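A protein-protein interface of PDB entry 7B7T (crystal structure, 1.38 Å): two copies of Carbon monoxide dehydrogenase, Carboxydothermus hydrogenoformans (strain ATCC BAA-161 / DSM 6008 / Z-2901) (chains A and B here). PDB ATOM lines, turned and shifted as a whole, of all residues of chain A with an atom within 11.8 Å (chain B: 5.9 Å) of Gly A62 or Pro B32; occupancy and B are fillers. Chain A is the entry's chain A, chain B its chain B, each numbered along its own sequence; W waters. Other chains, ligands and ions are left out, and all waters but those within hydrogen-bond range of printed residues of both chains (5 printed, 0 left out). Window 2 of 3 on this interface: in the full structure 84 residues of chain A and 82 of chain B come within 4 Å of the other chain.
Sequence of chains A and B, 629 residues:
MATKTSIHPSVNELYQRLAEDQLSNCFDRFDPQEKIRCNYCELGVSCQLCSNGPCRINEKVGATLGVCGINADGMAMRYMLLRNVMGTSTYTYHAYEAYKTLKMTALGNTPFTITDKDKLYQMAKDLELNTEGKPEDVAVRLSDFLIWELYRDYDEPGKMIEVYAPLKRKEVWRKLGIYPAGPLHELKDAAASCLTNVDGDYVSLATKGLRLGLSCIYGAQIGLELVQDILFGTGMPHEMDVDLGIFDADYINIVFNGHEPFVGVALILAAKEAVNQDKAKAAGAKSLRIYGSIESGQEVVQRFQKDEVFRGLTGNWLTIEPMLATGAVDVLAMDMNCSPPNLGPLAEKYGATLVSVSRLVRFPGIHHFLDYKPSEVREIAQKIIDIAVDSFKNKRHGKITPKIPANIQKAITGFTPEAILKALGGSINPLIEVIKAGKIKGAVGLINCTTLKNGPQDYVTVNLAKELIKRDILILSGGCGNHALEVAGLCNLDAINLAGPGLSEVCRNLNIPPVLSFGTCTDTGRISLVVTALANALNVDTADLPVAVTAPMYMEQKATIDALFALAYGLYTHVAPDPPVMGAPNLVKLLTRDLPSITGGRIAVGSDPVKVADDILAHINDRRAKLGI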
ATOM      1  N   TYR A  40     -13.016  20.767  -4.878  1.00  0.00           N
ATOM      2  CA  TYR A  40     -13.760  19.863  -5.749  1.00  0.00           C
ATOM      3  C   TYR A  40     -14.050  20.525  -7.082  1.00  0.00           C
ATOM      4  O   TYR A  40     -13.818  19.939  -8.158  1.00  0.00           O
ATOM      5  CB  TYR A  40     -15.061  19.424  -5.096  1.00  0.00           C
ATOM      6  CG  TYR A  40     -14.898  18.593  -3.841  1.00  0.00           C
ATOM      7  CD1 TYR A  40     -14.772  17.212  -3.898  1.00  0.00           C
ATOM      8  CD2 TYR A  40     -14.895  19.191  -2.579  1.00  0.00           C
ATOM      9  CE1 TYR A  40     -14.632  16.461  -2.747  1.00  0.00           C
ATOM     10  CE2 TYR A  40     -14.771  18.427  -1.410  1.00  0.00           C
ATOM     11  CZ  TYR A  40     -14.646  17.064  -1.515  1.00  0.00           C
ATOM     12  OH  TYR A  40     -14.530  16.275  -0.400  1.00  0.00           O
ATOM     13  N   VAL A  45     -14.673  17.856 -10.061  1.00  0.00           N
ATOM     14  CA  VAL A  45     -15.278  16.667  -9.477  1.00  0.00           C
ATOM     15  C   VAL A  45     -16.387  16.994  -8.495  1.00  0.00           C
ATOM     16  O   VAL A  45     -16.549  16.332  -7.466  1.00  0.00           O
ATOM     17  CB  VAL A  45     -14.226  15.721  -8.878  1.00  0.00           C
ATOM     18  CG1 VAL A  45     -13.370  15.155  -9.990  1.00  0.00           C
ATOM     19  CG2 VAL A  45     -13.357  16.390  -7.778  1.00  0.00           C
ATOM     20  N   ASN A  52     -30.838  14.963  -6.694  1.00  0.00           N
ATOM     21  CA  ASN A  52     -30.172  14.000  -5.825  1.00  0.00           C
ATOM     22  C   ASN A  52     -28.833  14.517  -5.327  1.00  0.00           C
ATOM     23  O   ASN A  52     -28.282  13.953  -4.370  1.00  0.00           O
ATOM     24  CB  ASN A  52     -29.977  12.639  -6.510  1.00  0.00           C
ATOM     25  CG  ASN A  52     -31.156  11.679  -6.307  1.00  0.00           C
ATOM     26  OD1 ASN A  52     -31.756  11.601  -5.243  1.00  0.00           O
ATOM     27  ND2 ASN A  52     -31.441  10.897  -7.327  1.00  0.00           N
ATOM     28  N   GLY A  53     -28.278  15.518  -6.002  1.00  0.00           N
ATOM     29  CA  GLY A  53     -27.052  16.162  -5.605  1.00  0.00           C
ATOM     30  C   GLY A  53     -27.301  17.210  -4.553  1.00  0.00           C
ATOM     31  O   GLY A  53     -28.337  17.214  -3.885  1.00  0.00           O
ATOM     32  N   PRO A  54     -26.376  18.150  -4.415  1.00  0.00           N
ATOM     33  CA  PRO A  54     -25.124  18.247  -5.174  1.00  0.00           C
ATOM     34  C   PRO A  54     -24.173  17.106  -4.790  1.00  0.00           C
ATOM     35  O   PRO A  54     -24.219  16.617  -3.667  1.00  0.00           O
ATOM     36  CB  PRO A  54     -24.582  19.595  -4.749  1.00  0.00           C
ATOM     37  CG  PRO A  54     -25.137  19.805  -3.374  1.00  0.00           C
ATOM     38  CD  PRO A  54     -26.486  19.176  -3.373  1.00  0.00           C
ATOM     39  N   CYS A  55     -23.339  16.681  -5.719  1.00  0.00           N
ATOM     40  CA  CYS A  55     -22.447  15.552  -5.528  1.00  0.00           C
ATOM     41  C   CYS A  55     -20.988  15.969  -5.658  1.00  0.00           C
ATOM     42  O   CYS A  55     -20.658  16.993  -6.260  1.00  0.00           O
ATOM     43  CB  CYS A  55     -22.753  14.454  -6.557  1.00  0.00           C
ATOM     44  SG  CYS A  55     -24.323  13.660  -6.330  1.00  0.00           S
ATOM     45  N   ARG A  56     -20.130  15.143  -5.062  1.00  0.00           N
ATOM     46  CA  ARG A  56     -18.687  15.294  -5.045  1.00  0.00           C
ATOM     47  C   ARG A  56     -18.065  13.915  -5.170  1.00  0.00           C
ATOM     48  O   ARG A  56     -18.596  12.940  -4.637  1.00  0.00           O
ATOM     49  CB  ARG A  56     -18.230  15.889  -3.705  1.00  0.00           C
ATOM     50  CG  ARG A  56     -18.544  17.361  -3.589  1.00  0.00           C
ATOM     51  CD  ARG A  56     -18.420  17.828  -2.162  1.00  0.00           C
ATOM     52  NE  ARG A  56     -18.216  19.253  -2.113  1.00  0.00           N
ATOM     53  CZ  ARG A  56     -17.934  19.940  -1.014  1.00  0.00           C
ATOM     54  NH1 ARG A  56     -17.949  19.334   0.147  1.00  0.00           N
ATOM     55  NH2 ARG A  56     -17.681  21.246  -1.093  1.00  0.00           N
ATOM     56  N   ILE A  57     -16.929  13.830  -5.864  1.00  0.00           N
ATOM     57  CA  ILE A  57     -16.147  12.600  -5.853  1.00  0.00           C
ATOM     58  C   ILE A  57     -15.105  12.693  -4.752  1.00  0.00           C
ATOM     59  O   ILE A  57     -14.236  13.562  -4.786  1.00  0.00           O
ATOM     60  CB  ILE A  57     -15.490  12.313  -7.207  1.00  0.00           C
ATOM     61  CG1 ILE A  57     -16.539  12.328  -8.332  1.00  0.00           C
ATOM     62  CG2 ILE A  57     -14.780  10.966  -7.155  1.00  0.00           C
ATOM     63  CD1 ILE A  57     -17.631  11.290  -8.180  1.00  0.00           C
ATOM     64  N   ASN A  58     -15.184  11.782  -3.790  1.00  0.00           N
ATOM     65  CA  ASN A  58     -14.197  11.682  -2.721  1.00  0.00           C
ATOM     66  C   ASN A  58     -14.140  10.206  -2.340  1.00  0.00           C
ATOM     67  O   ASN A  58     -14.963   9.728  -1.549  1.00  0.00           O
ATOM     68  CB  ASN A  58     -14.592  12.560  -1.542  1.00  0.00           C
ATOM     69  CG  ASN A  58     -13.525  12.631  -0.489  1.00  0.00           C
ATOM     70  OD1 ASN A  58     -12.716  11.717  -0.340  1.00  0.00           O
ATOM     71  ND2 ASN A  58     -13.525  13.722   0.267  1.00  0.00           N
ATOM     72  N   GLU A  59     -13.185   9.488  -2.928  1.00  0.00           N
ATOM     73  CA  GLU A  59     -13.124   8.046  -2.725  1.00  0.00           C
ATOM     74  C   GLU A  59     -12.775   7.698  -1.286  1.00  0.00           C
ATOM     75  O   GLU A  59     -13.210   6.657  -0.793  1.00  0.00           O
ATOM     76  CB  GLU A  59     -12.168   7.417  -3.749  1.00  0.00           C
ATOM     77  CG  GLU A  59     -12.731   7.487  -5.177  1.00  0.00           C
ATOM     78  CD  GLU A  59     -11.927   6.707  -6.206  1.00  0.00           C
ATOM     79  OE1 GLU A  59     -11.806   5.470  -6.059  1.00  0.00           O
ATOM     80  OE2 GLU A  59     -11.428   7.331  -7.170  1.00  0.00           O
ATOM     81  N   LYS A  60     -12.085   8.596  -0.574  1.00  0.00           N
ATOM     82  CA  LYS A  60     -11.649   8.311   0.792  1.00  0.00           C
ATOM     83  C   LYS A  60     -12.821   8.122   1.745  1.00  0.00           C
ATOM     84  O   LYS A  60     -12.694   7.416   2.755  1.00  0.00           O
ATOM     85  CB  LYS A  60     -10.742   9.438   1.307  1.00  0.00           C
ATOM     86  CG  LYS A  60      -9.266   9.164   1.135  1.00  0.00           C
ATOM     87  CD  LYS A  60      -8.402  10.170   1.903  1.00  0.00           C
ATOM     88  CE  LYS A  60      -7.009   9.603   2.209  1.00  0.00           C
ATOM     89  NZ  LYS A  60      -6.972   8.919   3.533  1.00  0.00           N
ATOM     90  N   VAL A  61     -13.952   8.754   1.459  1.00  0.00           N
ATOM     91  CA  VAL A  61     -15.144   8.635   2.278  1.00  0.00           C
ATOM     92  C   VAL A  61     -16.228   7.841   1.557  1.00  0.00           C
ATOM     93  O   VAL A  61     -17.403   7.932   1.906  1.00  0.00           O
ATOM     94  CB  VAL A  61     -15.638  10.008   2.752  1.00  0.00           C
ATOM     95  CG1 VAL A  61     -14.535  10.697   3.578  1.00  0.00           C
ATOM     96  CG2 VAL A  61     -16.061  10.871   1.564  1.00  0.00           C
ATOM     97  N   GLY A  62     -15.847   7.088   0.529  1.00  0.00           N
ATOM     98  CA  GLY A  62     -16.772   6.188  -0.129  1.00  0.00           C
ATOM     99  C   GLY A  62     -17.633   6.806  -1.207  1.00  0.00           C
ATOM    100  O   GLY A  62     -18.543   6.133  -1.705  1.00  0.00           O
ATOM    101  N   ALA A  63     -17.393   8.063  -1.565  1.00  0.00           N
ATOM    102  CA  ALA A  63     -18.166   8.763  -2.578  1.00  0.00           C
ATOM    103  C   ALA A  63     -17.435   8.679  -3.916  1.00  0.00           C
ATOM    104  O   ALA A  63     -16.897   9.648  -4.443  1.00  0.00           O
ATOM    105  CB  ALA A  63     -18.403  10.210  -2.151  1.00  0.00           C
ATOM    106  N   THR A  64     -17.417   7.470  -4.448  1.00  0.00           N
ATOM    107  CA  THR A  64     -16.707   7.169  -5.683  1.00  0.00           C
ATOM    108  C   THR A  64     -17.491   7.598  -6.916  1.00  0.00           C
ATOM    109  O   THR A  64     -16.893   7.897  -7.954  1.00  0.00           O
ATOM    110  CB  THR A  64     -16.428   5.675  -5.718  1.00  0.00           C
ATOM    111  OG1 THR A  64     -15.551   5.365  -4.626  1.00  0.00           O
ATOM    112  CG2 THR A  64     -15.798   5.294  -7.027  1.00  0.00           C
ATOM    113  N   LEU A  65     -18.812   7.603  -6.826  1.00  0.00           N
ATOM    114  CA  LEU A  65     -19.706   7.944  -7.913  1.00  0.00           C
ATOM    115  C   LEU A  65     -20.781   8.906  -7.399  1.00  0.00           C
ATOM    116  O   LEU A  65     -21.078   8.957  -6.208  1.00  0.00           O
ATOM    117  CB  LEU A  65     -20.415   6.683  -8.416  1.00  0.00           C
ATOM    118  CG  LEU A  65     -19.526   5.540  -8.891  1.00  0.00           C
ATOM    119  CD1 LEU A  65     -20.402   4.308  -9.253  1.00  0.00           C
ATOM    120  CD2 LEU A  65     -18.645   5.924 -10.093  1.00  0.00           C
ATOM    121  N   GLY A  66     -21.345   9.693  -8.300  1.00  0.00           N
ATOM    122  CA  GLY A  66     -22.537  10.455  -7.984  1.00  0.00           C
ATOM    123  C   GLY A  66     -23.690   9.531  -7.613  1.00  0.00           C
ATOM    124  O   GLY A  66     -23.662   8.331  -7.842  1.00  0.00           O
ATOM    125  N   VAL A  67     -24.752  10.116  -7.061  1.00  0.00           N
ATOM    126  CA  VAL A  67     -25.907   9.304  -6.702  1.00  0.00           C
ATOM    127  C   VAL A  67     -26.412   8.521  -7.911  1.00  0.00           C
ATOM    128  O   VAL A  67     -26.757   7.347  -7.806  1.00  0.00           O
ATOM    129  CB  VAL A  67     -27.016  10.153  -6.047  1.00  0.00           C
ATOM    130  CG1 VAL A  67     -28.238   9.277  -5.736  1.00  0.00           C
ATOM    131  CG2 VAL A  67     -26.515  10.858  -4.764  1.00  0.00           C
ATOM    132  N   CYS A  68     -26.466   9.175  -9.069  1.00  0.00           N
ATOM    133  CA  CYS A  68     -26.929   8.555 -10.306  1.00  0.00           C
ATOM    134  C   CYS A  68     -26.013   7.452 -10.820  1.00  0.00           C
ATOM    135  O   CYS A  68     -26.441   6.670 -11.680  1.00  0.00           O
ATOM    136  CB  CYS A  68     -27.050   9.607 -11.403  1.00  0.00           C
ATOM    137  SG  CYS A  68     -25.462  10.450 -11.747  1.00  0.00           S
ATOM    138  N   GLY A  69     -24.762   7.392 -10.371  1.00  0.00           N
ATOM    139  CA  GLY A  69     -23.802   6.396 -10.798  1.00  0.00           C
ATOM    140  C   GLY A  69     -22.691   6.934 -11.684  1.00  0.00           C
ATOM    141  O   GLY A  69     -21.827   6.163 -12.078  1.00  0.00           O
ATOM    142  N   ILE A  70     -22.663   8.230 -11.990  1.00  0.00           N
ATOM    143  CA  ILE A  70     -21.638   8.741 -12.892  1.00  0.00           C
ATOM    144  C   ILE A  70     -20.287   8.801 -12.169  1.00  0.00           C
ATOM    145  O   ILE A  70     -20.200   9.050 -10.944  1.00  0.00           O
ATOM    146  CB  ILE A  70     -22.046  10.113 -13.462  1.00  0.00           C
ATOM    147  CG1 ILE A  70     -21.231  10.441 -14.718  1.00  0.00           C
ATOM    148  CG2 ILE A  70     -21.902  11.221 -12.412  1.00  0.00           C
ATOM    149  CD1 ILE A  70     -21.741  11.665 -15.499  1.00  0.00           C
ATOM    150  N   ASN A  71     -19.218   8.563 -12.930  1.00  0.00           N
ATOM    151  CA  ASN A  71     -17.858   8.629 -12.395  1.00  0.00           C
ATOM    152  C   ASN A  71     -17.239  10.010 -12.628  1.00  0.00           C
ATOM    153  O   ASN A  71     -17.814  10.870 -13.291  1.00  0.00           O
ATOM    154  CB  ASN A  71     -16.982   7.475 -12.897  1.00  0.00           C
ATOM    155  CG  ASN A  71     -16.741   7.486 -14.404  1.00  0.00           C
ATOM    156  OD1 ASN A  71     -16.575   8.536 -15.039  1.00  0.00           O
ATOM    157  ND2 ASN A  71     -16.647   6.303 -14.967  1.00  0.00           N
ATOM    158  N   ALA A  72     -16.062  10.224 -12.031  1.00  0.00           N
ATOM    159  CA  ALA A  72     -15.388  11.524 -12.096  1.00  0.00           C
ATOM    160  C   ALA A  72     -15.130  11.961 -13.526  1.00  0.00           C
ATOM    161  O   ALA A  72     -15.230  13.156 -13.838  1.00  0.00           O
ATOM    162  CB  ALA A  72     -14.051  11.458 -11.369  1.00  0.00           C
ATOM    163  N   MET A  75     -18.340  13.037 -15.093  1.00  0.00           N
ATOM    164  CA  MET A  75     -18.786  14.263 -14.440  1.00  0.00           C
ATOM    165  C   MET A  75     -18.055  15.480 -14.984  1.00  0.00           C
ATOM    166  O   MET A  75     -18.680  16.487 -15.352  1.00  0.00           O
ATOM    167  CB  MET A  75     -18.582  14.116 -12.926  1.00  0.00           C
ATOM    168  CG  MET A  75     -19.019  15.293 -12.109  1.00  0.00           C
ATOM    169  SD  MET A  75     -18.707  15.053 -10.319  1.00  0.00           S
ATOM    170  CE  MET A  75     -19.843  13.715  -9.965  1.00  0.00           C
ATOM    171  N   ASP B  28     -27.791   3.121  -2.077  1.00  0.00           N
ATOM    172  CA  ASP B  28     -26.576   3.094  -1.281  1.00  0.00           C
ATOM    173  C   ASP B  28     -25.647   4.259  -1.593  1.00  0.00           C
ATOM    174  O   ASP B  28     -24.903   4.696  -0.709  1.00  0.00           O
ATOM    175  CB  ASP B  28     -25.850   1.759  -1.439  1.00  0.00           C
ATOM    176  CG  ASP B  28     -26.582   0.613  -0.732  1.00  0.00           C
ATOM    177  OD1 ASP B  28     -27.264   0.865   0.296  1.00  0.00           O
ATOM    178  OD2 ASP B  28     -26.481  -0.543  -1.200  1.00  0.00           O
ATOM    179  N   ARG B  29     -25.658   4.766  -2.833  1.00  0.00           N
ATOM    180  CA  ARG B  29     -24.768   5.868  -3.191  1.00  0.00           C
ATOM    181  C   ARG B  29     -25.207   7.187  -2.579  1.00  0.00           C
ATOM    182  O   ARG B  29     -24.403   8.123  -2.515  1.00  0.00           O
ATOM    183  CB  ARG B  29     -24.649   6.014  -4.710  1.00  0.00           C
ATOM    184  CG  ARG B  29     -23.848   4.922  -5.355  1.00  0.00           C
ATOM    185  CD  ARG B  29     -23.598   5.200  -6.835  1.00  0.00           C
ATOM    186  NE  ARG B  29     -24.832   5.269  -7.622  1.00  0.00           N
ATOM    187  CZ  ARG B  29     -25.333   4.305  -8.369  1.00  0.00           C
ATOM    188  NH1 ARG B  29     -24.700   3.146  -8.477  1.00  0.00           N
ATOM    189  NH2 ARG B  29     -26.456   4.537  -9.052  1.00  0.00           N
ATOM    190  N   PHE B  30     -26.453   7.275  -2.120  1.00  0.00           N
ATOM    191  CA  PHE B  30     -26.953   8.527  -1.568  1.00  0.00           C
ATOM    192  C   PHE B  30     -26.226   8.913  -0.287  1.00  0.00           C
ATOM    193  O   PHE B  30     -25.866  10.088  -0.106  1.00  0.00           O
ATOM    194  CB  PHE B  30     -28.455   8.416  -1.315  1.00  0.00           C
ATOM    195  CG  PHE B  30     -29.118   9.713  -0.994  1.00  0.00           C
ATOM    196  CD1 PHE B  30     -29.576  10.562  -1.984  1.00  0.00           C
ATOM    197  CD2 PHE B  30     -29.278  10.087   0.315  1.00  0.00           C
ATOM    198  CE1 PHE B  30     -30.177  11.747  -1.656  1.00  0.00           C
ATOM    199  CE2 PHE B  30     -29.876  11.270   0.643  1.00  0.00           C
ATOM    200  CZ  PHE B  30     -30.326  12.095  -0.319  1.00  0.00           C
ATOM    201  N   ASP B  31     -25.988   7.953   0.628  1.00  0.00           N
ATOM    202  CA  ASP B  31     -25.480   8.395   1.928  1.00  0.00           C
ATOM    203  C   ASP B  31     -24.035   8.869   1.865  1.00  0.00           C
ATOM    204  O   ASP B  31     -23.708   9.838   2.547  1.00  0.00           O
ATOM    205  CB  ASP B  31     -25.698   7.478   3.122  1.00  0.00           C
ATOM    206  CG  ASP B  31     -25.691   8.278   4.450  1.00  0.00           C
ATOM    207  OD1 ASP B  31     -26.743   8.884   4.820  1.00  0.00           O
ATOM    208  OD2 ASP B  31     -24.625   8.342   5.105  1.00  0.00           O
ATOM    209  N   PRO B  32     -23.134   8.244   1.097  1.00  0.00           N
ATOM    210  CA  PRO B  32     -21.788   8.830   1.015  1.00  0.00           C
ATOM    211  C   PRO B  32     -21.813  10.263   0.528  1.00  0.00           C
ATOM    212  O   PRO B  32     -21.002  11.062   0.999  1.00  0.00           O
ATOM    213  CB  PRO B  32     -21.020   7.883   0.090  1.00  0.00           C
ATOM    214  CG  PRO B  32     -21.766   6.610   0.166  1.00  0.00           C
ATOM    215  CD  PRO B  32     -23.196   6.943   0.407  1.00  0.00           C
ATOM    216  N   GLN B  33     -22.743  10.623  -0.367  1.00  0.00           N
ATOM    217  CA  GLN B  33     -22.851  12.013  -0.810  1.00  0.00           C
ATOM    218  C   GLN B  33     -23.419  12.887   0.295  1.00  0.00           C
ATOM    219  O   GLN B  33     -22.996  14.039   0.467  1.00  0.00           O
ATOM    220  CB  GLN B  33     -23.734  12.099  -2.066  1.00  0.00           C
ATOM    221  CG  GLN B  33     -23.113  11.476  -3.283  1.00  0.00           C
ATOM    222  CD  GLN B  33     -21.858  12.199  -3.731  1.00  0.00           C
ATOM    223  OE1 GLN B  33     -21.647  13.339  -3.387  1.00  0.00           O
ATOM    224  NE2 GLN B  33     -21.022  11.525  -4.494  1.00  0.00           N
ATOM    225  N   GLU B  34     -24.401  12.356   1.031  1.00  0.00           N
ATOM    226  CA  GLU B  34     -24.920  13.039   2.214  1.00  0.00           C
ATOM    227  C   GLU B  34     -23.797  13.513   3.118  1.00  0.00           C
ATOM    228  O   GLU B  34     -23.854  14.629   3.662  1.00  0.00           O
ATOM    229  CB  GLU B  34     -25.832  12.087   2.994  1.00  0.00           C
ATOM    230  CG  GLU B  34     -27.163  11.875   2.326  1.00  0.00           C
ATOM    231  CD  GLU B  34     -28.026  13.100   2.450  1.00  0.00           C
ATOM    232  OE1 GLU B  34     -28.744  13.220   3.464  1.00  0.00           O
ATOM    233  OE2 GLU B  34     -27.946  13.954   1.550  1.00  0.00           O
ATOM    234  N   LYS B  35     -22.775  12.673   3.307  1.00  0.00           N
ATOM    235  CA  LYS B  35     -21.743  12.952   4.299  1.00  0.00           C
ATOM    236  C   LYS B  35     -20.907  14.180   3.949  1.00  0.00           C
ATOM    237  O   LYS B  35     -20.277  14.759   4.844  1.00  0.00           O
ATOM    238  CB  LYS B  35     -20.830  11.728   4.468  1.00  0.00           C
ATOM    239  CG  LYS B  35     -21.434  10.563   5.281  1.00  0.00           C
ATOM    240  CD  LYS B  35     -20.560   9.289   5.213  1.00  0.00           C
ATOM    241  CE  LYS B  35     -19.397   9.307   6.221  1.00  0.00           C
ATOM    242  NZ  LYS B  35     -19.842   9.208   7.631  1.00  0.00           N
ATOM    243  N   ILE B  36     -20.878  14.579   2.679  1.00  0.00           N
ATOM    244  CA  ILE B  36     -19.982  15.646   2.249  1.00  0.00           C
ATOM    245  C   ILE B  36     -20.702  16.737   1.463  1.00  0.00           C
ATOM    246  O   ILE B  36     -20.065  17.478   0.705  1.00  0.00           O
ATOM    247  CB  ILE B  36     -18.752  15.109   1.486  1.00  0.00           C
ATOM    248  CG1 ILE B  36     -19.147  14.294   0.248  1.00  0.00           C
ATOM    249  CG2 ILE B  36     -17.852  14.301   2.425  1.00  0.00           C
ATOM    250  CD1 ILE B  36     -17.927  13.855  -0.609  1.00  0.00           C
HETATM  251  O   HOH W   1     -21.912  15.621  -1.784  1.00  0.00           O
HETATM  252  O   HOH W   2     -26.400   3.920 -12.286  1.00  0.00           O
HETATM  253  O   HOH W   3     -17.613  18.016   3.142  1.00  0.00           O
HETATM  254  O   HOH W   4     -18.977  10.078   2.467  1.00  0.00           O
HETATM  255  O   HOH W   5     -21.798   7.976  -3.659  1.00  0.00           O
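O of Cys A68 is in hydrogen-bond range of NH2 of Arg B29 (3.4 Å). O of Gly A66 sits at hydrogen-bond distance from NE of Arg B29, at 3.3 Å. NH1 of Arg A56 sits at hydrogen-bond distance from O of Ile B36 (2.9 Å). The backbone NH (N) of Gly A69 sits close to the guanidinium group (NE) of Arg B29 (3.5 Å). The backbone carbonyl oxygen of Val A67 is in hydrogen-bond range of the guanidinium group of Arg B29 (2.8 Å). NE2 of Gln B33 is in hydrogen-bond range of O of Leu A65, 3.1 Å away. The side-chain amide nitrogen (NE2) of Gln B33 lies within hydrogen-bond range of the backbone carbonyl oxygen (O) of Arg A56, 2.8 Å away.
N of Asn A58 lies within hydrogen-bond range of O of Ala A63. SG of Cys A68 sits close to N of Ile A70 (3.6 Å). The side-chain amide oxygen (OD1) of Asn A58 sits close to the backbone NH (N) of Lys A60, 3.2 Å away. The side-chain sulfur (SG) of Cys A55 lies close to the backbone NH (N) of Val A67. The side-chain hydroxyl of Tyr A40 sits at hydrogen-bond distance from the side-chain amide nitrogen of Asn A58 (2.8 Å).
Phe B30 touches Asn A52 (CE1 to OD1, 3.9 Å). Cys A55 touches Gln B33 (CA to OE1, 3.2 Å). Asn A58 touches Ile B36 (CB to CD1, 3.7 Å). Gly A62 touches Pro B32. Ala A63 touches Pro B32 (N to CB, 3.99 Å). Ala A63 touches Gln B33. CD1 of Ile B36 touches CB of Ala A63, at 3.99 Å. Gln B33 touches Gly A66 (NE2 to CA, 3.95 Å). Val A67 touches Phe B30. Val A67 touches Gln B33.
Printed residues of chain B within 4 Å of Val A61: Ile B36 (3.96 Å). Of the printed residues of chain B, Val A67 touches Arg B29, Phe B30 and Gln B33. Printed residues of chain A within 4 Å of Phe B30: Asn A52 (3.9 Å) and Val A67 (3.98 Å). Of the printed residues of chain A, Pro B32 touches Gly A62 (3.5 Å) and Ala A63 (3.99 Å). Gln B33 touches six residues of chain A. Printed residues of chain A within 4 Å of Ile B36: Arg A56, Asn A58, Val A61 and Ala A63. The nearest printed residue of chain B that does not touch Gly A62 is Arg B29 (6.2 Å).
Hydrophobic or aromatic side chains of chain A within 4 Å of the printed part of chain B: Val A61, Ala A63, Leu A65 and Val A67. Of the 9 printed residues of chain B, 5 touch a printed residue of chain A. Hydrophobic or aromatic side chains of chain B within 4 Å of the printed part of chain A: Phe B30, Pro B32 and Ile B36.
No position is printed for both chains. Of the 19 pairs that touch across the chains among the printed residues, none has its exchanged pair printed and touching as well.
Water W4 bridges O of Pro B32 and O of Val A61. Water W1 lies within hydrogen-bond range of the side-chain amide oxygen (OE1) of Gln B33 (2.8 Å) and the backbone carbonyl oxygen (O) of Pro A54 (3.1 Å). Water W2 lies within hydrogen-bond range of O of Cys A68 and NH2 of Arg B29. Water W5 lies within hydrogen-bond range of the backbone carbonyl oxygen (O) of Leu A65 (2.8 Å) and the backbone carbonyl oxygen (O) of Arg B29 (2.8 Å). Water W3 lies within hydrogen-bond range of the guanidinium group (NH1) of Arg A56 (3.3 Å) and the backbone carbonyl oxygen (O) of Ile B36 (3.5 Å).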
